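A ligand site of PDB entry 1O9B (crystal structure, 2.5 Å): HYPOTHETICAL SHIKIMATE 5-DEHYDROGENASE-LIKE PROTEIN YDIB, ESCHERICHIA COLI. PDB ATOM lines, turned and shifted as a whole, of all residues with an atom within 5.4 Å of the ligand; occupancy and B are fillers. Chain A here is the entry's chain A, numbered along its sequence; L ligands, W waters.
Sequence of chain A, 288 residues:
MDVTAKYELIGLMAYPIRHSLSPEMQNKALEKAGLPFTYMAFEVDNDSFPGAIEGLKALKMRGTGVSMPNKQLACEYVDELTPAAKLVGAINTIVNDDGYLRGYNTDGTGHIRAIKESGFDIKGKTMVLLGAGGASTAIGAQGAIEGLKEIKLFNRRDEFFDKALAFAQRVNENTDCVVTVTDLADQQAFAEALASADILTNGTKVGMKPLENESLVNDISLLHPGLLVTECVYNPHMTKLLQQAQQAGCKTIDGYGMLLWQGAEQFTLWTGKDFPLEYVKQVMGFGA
Residues that only touch the ligand: Tyr 234 (3.1 Å), Phe 160 (3.2 Å), Met 258 (3.3 Å), Gly 203 (3.4 Å), Thr 204 (3.6 Å), Val 206 (3.7 Å), Val 233 (3.7 Å) and Asp 107 (3.8 Å). Hydrophobic or aromatic side chains that line the ligand: Ala 135, Phe 160, Val 206, Met 208, Val 233, Tyr 234, Met 258 and Leu 259.
The backbone NH of Gly 133 lies within hydrogen-bond range of an oxygen (O5) of the ligand (2.5 Å). An oxygen (O9) of the ligand sits at hydrogen-bond distance from the backbone NH (N) of Gly 134 (2.5 Å). N of Ala 135 sits at hydrogen-bond distance from O9 of the ligand, at 2.7 Å. The side-chain amino group of Lys 205 is in salt-bridge range of an oxygen (O2) of the ligand. N7 of the ligand sits close to O of Cys 232 (3.0 Å). A nitrogen (N4) of the ligand lies close to the guanidinium group of Arg 156 (3.2 Å). The backbone NH (N) of Ala 132 is in hydrogen-bond range of an oxygen (O5) of the ligand, at 3.0 Å. The backbone carbonyl oxygen (O) of Gly 255 sits at hydrogen-bond distance from a nitrogen (N7) of the ligand (3.2 Å). An oxygen (O12) of the ligand sits close to the side-chain sulfur (SD) of Met 208. An oxygen (O14) of the ligand sits close to the backbone NH (N) of Leu 259 (3.4 Å). OD1 of Asn 155 is in hydrogen-bond range of O6 of the ligand, at 3.4 Å.
The side-chain amide oxygen (OD1) of Asn 155 is in hydrogen-bond range of the backbone NH (N) of Ala 132 (3.1 Å). O of Tyr 234 sits close to OH of Tyr 256 (3.2 Å). OE1 of Gln 262 lies close to O of Leu 259, at 3.4 Å. The backbone carbonyl oxygen of Gly 203 lies within hydrogen-bond range of the side-chain hydroxyl of Ser 136, at 3.2 Å. OD1 of Asn 155 sits close to O of Gly 131, 3.5 Å away. N of Val 206 lies close to OG1 of Thr 204.
Water W1 lies within hydrogen-bond range of the guanidinium group (NH1) of Arg 156 (2.6 Å) and a nitrogen (N3) of the ligand (2.8 Å). Water W2 lies within hydrogen-bond range of NZ of Lys 71 (2.9 Å) and O8 of the ligand (3.5 Å).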
ATOM      1  N   LYS A  71      27.620  -7.330 -12.735  1.00  0.00           N
ATOM      2  CA  LYS A  71      28.679  -7.844 -11.890  1.00  0.00           C
ATOM      3  C   LYS A  71      28.791  -9.363 -11.852  1.00  0.00           C
ATOM      4  O   LYS A  71      29.894  -9.918 -11.817  1.00  0.00           O
ATOM      5  CB  LYS A  71      28.520  -7.254 -10.479  1.00  0.00           C
ATOM      6  CG  LYS A  71      28.815  -5.753 -10.423  1.00  0.00           C
ATOM      7  CD  LYS A  71      28.201  -5.081  -9.198  1.00  0.00           C
ATOM      8  CE  LYS A  71      28.965  -5.366  -7.918  1.00  0.00           C
ATOM      9  NZ  LYS A  71      28.220  -4.825  -6.746  1.00  0.00           N
ATOM     10  N   ASP A 107      35.467  -3.939  -3.967  1.00  0.00           N
ATOM     11  CA  ASP A 107      34.632  -3.525  -2.852  1.00  0.00           C
ATOM     12  C   ASP A 107      35.195  -4.230  -1.632  1.00  0.00           C
ATOM     13  O   ASP A 107      35.399  -3.609  -0.602  1.00  0.00           O
ATOM     14  CB  ASP A 107      33.166  -3.945  -3.040  1.00  0.00           C
ATOM     15  CG  ASP A 107      32.421  -3.073  -4.050  1.00  0.00           C
ATOM     16  OD1 ASP A 107      32.617  -1.839  -4.016  1.00  0.00           O
ATOM     17  OD2 ASP A 107      31.643  -3.623  -4.848  1.00  0.00           O
ATOM     18  N   GLY A 131      23.968  -8.672   6.318  1.00  0.00           N
ATOM     19  CA  GLY A 131      23.654  -8.661   4.904  1.00  0.00           C
ATOM     20  C   GLY A 131      24.234  -9.857   4.182  1.00  0.00           C
ATOM     21  O   GLY A 131      24.945 -10.667   4.766  1.00  0.00           O
ATOM     22  N   ALA A 132      23.910  -9.972   2.903  1.00  0.00           N
ATOM     23  CA  ALA A 132      24.414 -11.060   2.075  1.00  0.00           C
ATOM     24  C   ALA A 132      24.353 -10.626   0.609  1.00  0.00           C
ATOM     25  O   ALA A 132      24.501 -11.438  -0.301  1.00  0.00           O
ATOM     26  N   GLY A 133      24.149  -9.319   0.430  1.00  0.00           N
ATOM     27  CA  GLY A 133      24.023  -8.706  -0.881  1.00  0.00           C
ATOM     28  C   GLY A 133      25.323  -8.587  -1.641  1.00  0.00           C
ATOM     29  O   GLY A 133      26.102  -9.527  -1.648  1.00  0.00           O
ATOM     30  N   GLY A 134      25.545  -7.435  -2.276  1.00  0.00           N
ATOM     31  CA  GLY A 134      26.765  -7.256  -3.046  1.00  0.00           C
ATOM     32  C   GLY A 134      27.923  -6.846  -2.162  1.00  0.00           C
ATOM     33  O   GLY A 134      29.016  -7.404  -2.230  1.00  0.00           O
ATOM     34  N   ALA A 135      27.658  -5.864  -1.303  1.00  0.00           N
ATOM     35  CA  ALA A 135      28.686  -5.365  -0.396  1.00  0.00           C
ATOM     36  C   ALA A 135      29.117  -6.446   0.590  1.00  0.00           C
ATOM     37  O   ALA A 135      30.292  -6.858   0.613  1.00  0.00           O
ATOM     38  CB  ALA A 135      28.156  -4.161   0.368  1.00  0.00           C
ATOM     39  N   SER A 136      28.164  -6.906   1.381  1.00  0.00           N
ATOM     40  CA  SER A 136      28.404  -7.926   2.402  1.00  0.00           C
ATOM     41  C   SER A 136      29.230  -9.152   1.988  1.00  0.00           C
ATOM     42  O   SER A 136      30.231  -9.483   2.611  1.00  0.00           O
ATOM     43  CB  SER A 136      27.075  -8.397   2.990  1.00  0.00           C
ATOM     44  OG  SER A 136      26.422  -7.335   3.669  1.00  0.00           O
ATOM     45  N   ASN A 155      21.516 -12.945   8.137  1.00  0.00           N
ATOM     46  CA  ASN A 155      20.643 -12.594   7.013  1.00  0.00           C
ATOM     47  C   ASN A 155      19.216 -13.135   7.235  1.00  0.00           C
ATOM     48  O   ASN A 155      19.024 -14.286   7.658  1.00  0.00           O
ATOM     49  CB  ASN A 155      21.226 -13.177   5.713  1.00  0.00           C
ATOM     50  CG  ASN A 155      20.952 -12.309   4.508  1.00  0.00           C
ATOM     51  OD1 ASN A 155      21.532 -11.237   4.347  1.00  0.00           O
ATOM     52  ND2 ASN A 155      20.061 -12.770   3.644  1.00  0.00           N
ATOM     53  N   ARG A 156      18.208 -12.317   6.929  1.00  0.00           N
ATOM     54  CA  ARG A 156      16.791 -12.685   7.119  1.00  0.00           C
ATOM     55  C   ARG A 156      16.193 -13.650   6.083  1.00  0.00           C
ATOM     56  O   ARG A 156      16.873 -14.117   5.170  1.00  0.00           O
ATOM     57  CB  ARG A 156      15.949 -11.406   7.177  1.00  0.00           C
ATOM     58  CG  ARG A 156      15.713 -10.785   5.809  1.00  0.00           C
ATOM     59  CD  ARG A 156      15.126  -9.392   5.909  1.00  0.00           C
ATOM     60  NE  ARG A 156      14.721  -8.920   4.578  1.00  0.00           N
ATOM     61  CZ  ARG A 156      14.237  -7.712   4.327  1.00  0.00           C
ATOM     62  NH1 ARG A 156      14.112  -6.835   5.316  1.00  0.00           N
ATOM     63  NH2 ARG A 156      13.885  -7.376   3.101  1.00  0.00           N
ATOM     64  N   PHE A 160      17.812 -13.259  -0.193  1.00  0.00           N
ATOM     65  CA  PHE A 160      19.238 -13.467   0.066  1.00  0.00           C
ATOM     66  C   PHE A 160      19.665 -14.577   1.017  1.00  0.00           C
ATOM     67  O   PHE A 160      20.821 -14.978   0.994  1.00  0.00           O
ATOM     68  CB  PHE A 160      19.887 -12.174   0.540  1.00  0.00           C
ATOM     69  CG  PHE A 160      19.749 -11.034  -0.445  1.00  0.00           C
ATOM     70  CD1 PHE A 160      18.573 -10.295  -0.530  1.00  0.00           C
ATOM     71  CD2 PHE A 160      20.795 -10.673  -1.272  1.00  0.00           C
ATOM     72  CE1 PHE A 160      18.477  -9.223  -1.411  1.00  0.00           C
ATOM     73  CE2 PHE A 160      20.690  -9.602  -2.150  1.00  0.00           C
ATOM     74  CZ  PHE A 160      19.537  -8.878  -2.204  1.00  0.00           C
ATOM     75  N   GLY A 203      26.448  -4.170   6.056  1.00  0.00           N
ATOM     76  CA  GLY A 203      26.467  -4.168   4.608  1.00  0.00           C
ATOM     77  C   GLY A 203      25.049  -4.152   4.082  1.00  0.00           C
ATOM     78  O   GLY A 203      24.795  -4.639   2.980  1.00  0.00           O
ATOM     79  N   THR A 204      24.136  -3.589   4.875  1.00  0.00           N
ATOM     80  CA  THR A 204      22.721  -3.506   4.485  1.00  0.00           C
ATOM     81  C   THR A 204      22.357  -2.106   4.050  1.00  0.00           C
ATOM     82  O   THR A 204      23.063  -1.158   4.379  1.00  0.00           O
ATOM     83  CB  THR A 204      21.790  -3.960   5.645  1.00  0.00           C
ATOM     84  OG1 THR A 204      21.673  -2.930   6.652  1.00  0.00           O
ATOM     85  CG2 THR A 204      22.306  -5.262   6.237  1.00  0.00           C
ATOM     86  N   LYS A 205      21.258  -1.991   3.298  1.00  0.00           N
ATOM     87  CA  LYS A 205      20.809  -0.701   2.790  1.00  0.00           C
ATOM     88  C   LYS A 205      20.265   0.116   3.946  1.00  0.00           C
ATOM     89  O   LYS A 205      20.061   1.337   3.822  1.00  0.00           O
ATOM     90  CB  LYS A 205      19.719  -0.901   1.727  1.00  0.00           C
ATOM     91  CG  LYS A 205      20.028  -2.025   0.740  1.00  0.00           C
ATOM     92  CD  LYS A 205      19.712  -1.607  -0.688  1.00  0.00           C
ATOM     93  CE  LYS A 205      19.483  -2.827  -1.558  1.00  0.00           C
ATOM     94  NZ  LYS A 205      19.895  -2.632  -2.974  1.00  0.00           N
ATOM     95  N   VAL A 206      20.065  -0.577   5.073  1.00  0.00           N
ATOM     96  CA  VAL A 206      19.546   0.038   6.291  1.00  0.00           C
ATOM     97  C   VAL A 206      20.472   1.114   6.811  1.00  0.00           C
ATOM     98  O   VAL A 206      21.625   0.846   7.119  1.00  0.00           O
ATOM     99  CB  VAL A 206      19.323  -1.036   7.372  1.00  0.00           C
ATOM    100  CG1 VAL A 206      18.443  -0.480   8.477  1.00  0.00           C
ATOM    101  CG2 VAL A 206      18.703  -2.301   6.759  1.00  0.00           C
ATOM    102  N   MET A 208      20.394   4.106   5.048  1.00  0.00           N
ATOM    103  CA  MET A 208      20.451   4.946   3.858  1.00  0.00           C
ATOM    104  C   MET A 208      19.092   5.506   3.415  1.00  0.00           C
ATOM    105  O   MET A 208      18.080   4.822   3.519  1.00  0.00           O
ATOM    106  CB  MET A 208      21.040   4.152   2.706  1.00  0.00           C
ATOM    107  CG  MET A 208      21.048   4.924   1.377  1.00  0.00           C
ATOM    108  SD  MET A 208      21.826   3.941  -0.126  1.00  0.00           S
ATOM    109  CE  MET A 208      20.819   2.268   0.008  1.00  0.00           C
ATOM    110  N   GLU A 214      17.176   4.138  10.693  1.00  0.00           N
ATOM    111  CA  GLU A 214      16.933   2.754  11.126  1.00  0.00           C
ATOM    112  C   GLU A 214      18.231   1.947  11.166  1.00  0.00           C
ATOM    113  O   GLU A 214      18.991   1.909  10.204  1.00  0.00           O
ATOM    114  CB  GLU A 214      15.885   2.072  10.226  1.00  0.00           C
ATOM    115  CG  GLU A 214      14.904   1.185  11.010  1.00  0.00           C
ATOM    116  CD  GLU A 214      13.830   0.579  10.179  1.00  0.00           C
ATOM    117  OE1 GLU A 214      14.122  -0.304   9.330  1.00  0.00           O
ATOM    118  OE2 GLU A 214      12.648   0.971  10.348  1.00  0.00           O
ATOM    119  N   LEU A 216      20.147  -1.879  12.524  1.00  0.00           N
ATOM    120  CA  LEU A 216      19.872  -3.276  12.776  1.00  0.00           C
ATOM    121  C   LEU A 216      20.240  -3.713  14.174  1.00  0.00           C
ATOM    122  O   LEU A 216      20.258  -4.917  14.475  1.00  0.00           O
ATOM    123  CB  LEU A 216      20.591  -4.152  11.756  1.00  0.00           C
ATOM    124  CG  LEU A 216      19.764  -4.493  10.522  1.00  0.00           C
ATOM    125  CD1 LEU A 216      19.061  -3.253  10.001  1.00  0.00           C
ATOM    126  CD2 LEU A 216      20.679  -5.076   9.472  1.00  0.00           C
ATOM    127  N   CYS A 232      29.012   0.509   5.441  1.00  0.00           N
ATOM    128  CA  CYS A 232      29.175   0.536   4.004  1.00  0.00           C
ATOM    129  C   CYS A 232      28.462   1.766   3.459  1.00  0.00           C
ATOM    130  O   CYS A 232      28.820   2.298   2.429  1.00  0.00           O
ATOM    131  CB  CYS A 232      28.601  -0.707   3.370  1.00  0.00           C
ATOM    132  SG  CYS A 232      29.726  -2.073   3.473  1.00  0.00           S
ATOM    133  N   VAL A 233      27.456   2.219   4.183  1.00  0.00           N
ATOM    134  CA  VAL A 233      26.693   3.379   3.755  1.00  0.00           C
ATOM    135  C   VAL A 233      27.489   4.653   3.902  1.00  0.00           C
ATOM    136  O   VAL A 233      28.077   4.920   4.954  1.00  0.00           O
ATOM    137  CB  VAL A 233      25.377   3.477   4.550  1.00  0.00           C
ATOM    138  CG1 VAL A 233      24.524   4.587   4.008  1.00  0.00           C
ATOM    139  CG2 VAL A 233      24.641   2.146   4.494  1.00  0.00           C
ATOM    140  N   TYR A 234      27.539   5.437   2.831  1.00  0.00           N
ATOM    141  CA  TYR A 234      28.254   6.694   2.862  1.00  0.00           C
ATOM    142  C   TYR A 234      27.286   7.839   2.618  1.00  0.00           C
ATOM    143  O   TYR A 234      27.690   8.999   2.475  1.00  0.00           O
ATOM    144  CB  TYR A 234      29.384   6.721   1.826  1.00  0.00           C
ATOM    145  CG  TYR A 234      28.962   6.554   0.387  1.00  0.00           C
ATOM    146  CD1 TYR A 234      28.308   7.578  -0.298  1.00  0.00           C
ATOM    147  CD2 TYR A 234      29.214   5.363  -0.291  1.00  0.00           C
ATOM    148  CE1 TYR A 234      27.916   7.422  -1.638  1.00  0.00           C
ATOM    149  CE2 TYR A 234      28.837   5.200  -1.618  1.00  0.00           C
ATOM    150  CZ  TYR A 234      28.191   6.216  -2.286  1.00  0.00           C
ATOM    151  OH  TYR A 234      27.818   6.027  -3.603  1.00  0.00           O
ATOM    152  N   GLY A 255      31.636   5.038   5.554  1.00  0.00           N
ATOM    153  CA  GLY A 255      31.456   4.642   4.183  1.00  0.00           C
ATOM    154  C   GLY A 255      32.486   5.237   3.234  1.00  0.00           C
ATOM    155  O   GLY A 255      32.919   4.558   2.303  1.00  0.00           O
ATOM    156  N   TYR A 256      32.882   6.482   3.461  1.00  0.00           N
ATOM    157  CA  TYR A 256      33.880   7.095   2.592  1.00  0.00           C
ATOM    158  C   TYR A 256      35.213   6.370   2.714  1.00  0.00           C
ATOM    159  O   TYR A 256      36.136   6.615   1.931  1.00  0.00           O
ATOM    160  CB  TYR A 256      34.043   8.565   2.958  1.00  0.00           C
ATOM    161  CG  TYR A 256      32.812   9.406   2.660  1.00  0.00           C
ATOM    162  CD1 TYR A 256      31.810   8.934   1.814  1.00  0.00           C
ATOM    163  CD2 TYR A 256      32.648  10.656   3.259  1.00  0.00           C
ATOM    164  CE1 TYR A 256      30.657   9.696   1.576  1.00  0.00           C
ATOM    165  CE2 TYR A 256      31.499  11.413   3.031  1.00  0.00           C
ATOM    166  CZ  TYR A 256      30.503  10.934   2.201  1.00  0.00           C
ATOM    167  OH  TYR A 256      29.359  11.674   1.986  1.00  0.00           O
ATOM    168  N   MET A 258      35.479   2.897   2.717  1.00  0.00           N
ATOM    169  CA  MET A 258      35.440   1.822   1.752  1.00  0.00           C
ATOM    170  C   MET A 258      35.396   2.413   0.351  1.00  0.00           C
ATOM    171  O   MET A 258      36.006   1.864  -0.571  1.00  0.00           O
ATOM    172  CB  MET A 258      34.217   0.931   1.978  1.00  0.00           C
ATOM    173  CG  MET A 258      34.121  -0.178   0.928  1.00  0.00           C
ATOM    174  SD  MET A 258      32.541  -1.253   1.052  1.00  0.00           S
ATOM    175  CE  MET A 258      31.496   0.017   2.009  1.00  0.00           C
ATOM    176  N   LEU A 259      34.721   3.542   0.190  1.00  0.00           N
ATOM    177  CA  LEU A 259      34.605   4.155  -1.125  1.00  0.00           C
ATOM    178  C   LEU A 259      35.941   4.674  -1.671  1.00  0.00           C
ATOM    179  O   LEU A 259      36.245   4.479  -2.845  1.00  0.00           O
ATOM    180  CB  LEU A 259      33.556   5.272  -1.091  1.00  0.00           C
ATOM    181  CG  LEU A 259      33.257   5.980  -2.405  1.00  0.00           C
ATOM    182  CD1 LEU A 259      33.023   4.978  -3.503  1.00  0.00           C
ATOM    183  CD2 LEU A 259      32.048   6.874  -2.231  1.00  0.00           C
ATOM    184  N   GLN A 262      38.500   1.544  -2.229  1.00  0.00           N
ATOM    185  CA  GLN A 262      37.992   0.712  -3.313  1.00  0.00           C
ATOM    186  C   GLN A 262      38.512   1.352  -4.606  1.00  0.00           C
ATOM    187  O   GLN A 262      39.077   0.672  -5.451  1.00  0.00           O
ATOM    188  CB  GLN A 262      36.456   0.720  -3.231  1.00  0.00           C
ATOM    189  CG  GLN A 262      35.703   0.218  -4.416  1.00  0.00           C
ATOM    190  CD  GLN A 262      35.634   1.229  -5.546  1.00  0.00           C
ATOM    191  OE1 GLN A 262      35.295   2.411  -5.340  1.00  0.00           O
ATOM    192  NE2 GLN A 262      35.934   0.764  -6.748  1.00  0.00           N
HETATM  193  P1  LIG L   1      22.129  -5.466  -2.386  1.00  0.00           P
HETATM  194  O1  LIG L   1      22.772  -6.553  -3.166  1.00  0.00           O
HETATM  195  O2  LIG L   1      20.747  -5.207  -2.827  1.00  0.00           O
HETATM  196  O3  LIG L   1      22.278  -5.960  -0.889  1.00  0.00           O
HETATM  197  C1  LIG L   1      21.521  -5.396   0.227  1.00  0.00           C
HETATM  198  C2  LIG L   1      21.570  -6.416   1.362  1.00  0.00           C
HETATM  199  O4  LIG L   1      20.821  -5.819   2.444  1.00  0.00           O
HETATM  200  C3  LIG L   1      20.879  -7.753   1.050  1.00  0.00           C
HETATM  201  O5  LIG L   1      21.805  -8.842   1.137  1.00  0.00           O
HETATM  202  C4  LIG L   1      19.679  -7.797   2.049  1.00  0.00           C
HETATM  203  O6  LIG L   1      19.522  -9.112   2.688  1.00  0.00           O
HETATM  204  C5  LIG L   1      19.996  -6.730   3.083  1.00  0.00           C
HETATM  205  N1  LIG L   1      18.835  -5.973   3.480  1.00  0.00           N
HETATM  206  C6  LIG L   1      18.129  -5.042   2.750  1.00  0.00           C
HETATM  207  N2  LIG L   1      17.091  -4.476   3.420  1.00  0.00           N
HETATM  208  C7  LIG L   1      17.168  -5.121   4.666  1.00  0.00           C
HETATM  209  C8  LIG L   1      16.362  -4.980   5.857  1.00  0.00           C
HETATM  210  N3  LIG L   1      15.325  -4.137   5.950  1.00  0.00           N
HETATM  211  N4  LIG L   1      16.717  -5.782   6.942  1.00  0.00           N
HETATM  212  C9  LIG L   1      17.796  -6.651   6.844  1.00  0.00           C
HETATM  213  N5  LIG L   1      18.587  -6.839   5.778  1.00  0.00           N
HETATM  214  C10 LIG L   1      18.235  -6.039   4.727  1.00  0.00           C
HETATM  215  O7  LIG L   1      22.947  -4.136  -2.422  1.00  0.00           O
HETATM  216  P2  LIG L   1      24.468  -3.798  -2.071  1.00  0.00           P
HETATM  217  O8  LIG L   1      25.044  -3.356  -3.384  1.00  0.00           O
HETATM  218  O9  LIG L   1      25.120  -5.023  -1.570  1.00  0.00           O
HETATM  219  O10 LIG L   1      24.553  -2.506  -1.156  1.00  0.00           O
HETATM  220  C11 LIG L   1      24.621  -2.631   0.294  1.00  0.00           C
HETATM  221  C12 LIG L   1      24.810  -1.240   0.907  1.00  0.00           C
HETATM  222  O11 LIG L   1      26.240  -0.927   0.827  1.00  0.00           O
HETATM  223  C13 LIG L   1      24.080  -0.082   0.219  1.00  0.00           C
HETATM  224  O12 LIG L   1      23.540   0.877   1.145  1.00  0.00           O
HETATM  225  C14 LIG L   1      25.163   0.517  -0.679  1.00  0.00           C
HETATM  226  O13 LIG L   1      24.852   1.914  -0.961  1.00  0.00           O
HETATM  227  C15 LIG L   1      26.420   0.283   0.142  1.00  0.00           C
HETATM  228  N6  LIG L   1      27.688   0.219  -0.664  1.00  0.00           N
HETATM  229  C16 LIG L   1      28.676   1.111  -0.254  1.00  0.00           C
HETATM  230  C17 LIG L   1      29.889   1.093  -0.958  1.00  0.00           C
HETATM  231  C18 LIG L   1      31.062   2.016  -0.598  1.00  0.00           C
HETATM  232  O14 LIG L   1      32.090   1.945  -1.251  1.00  0.00           O
HETATM  233  N7  LIG L   1      30.966   2.892   0.437  1.00  0.00           N
HETATM  234  C19 LIG L   1      30.113   0.174  -2.076  1.00  0.00           C
HETATM  235  C20 LIG L   1      29.010  -0.678  -2.398  1.00  0.00           C
HETATM  236  C21 LIG L   1      27.794  -0.713  -1.752  1.00  0.00           C
HETATM  237  O   HOH W   1      13.352  -4.620   4.089  1.00  0.00           O
HETATM  238  O   HOH W   2      25.377  -5.103  -6.341  1.00  0.00           O
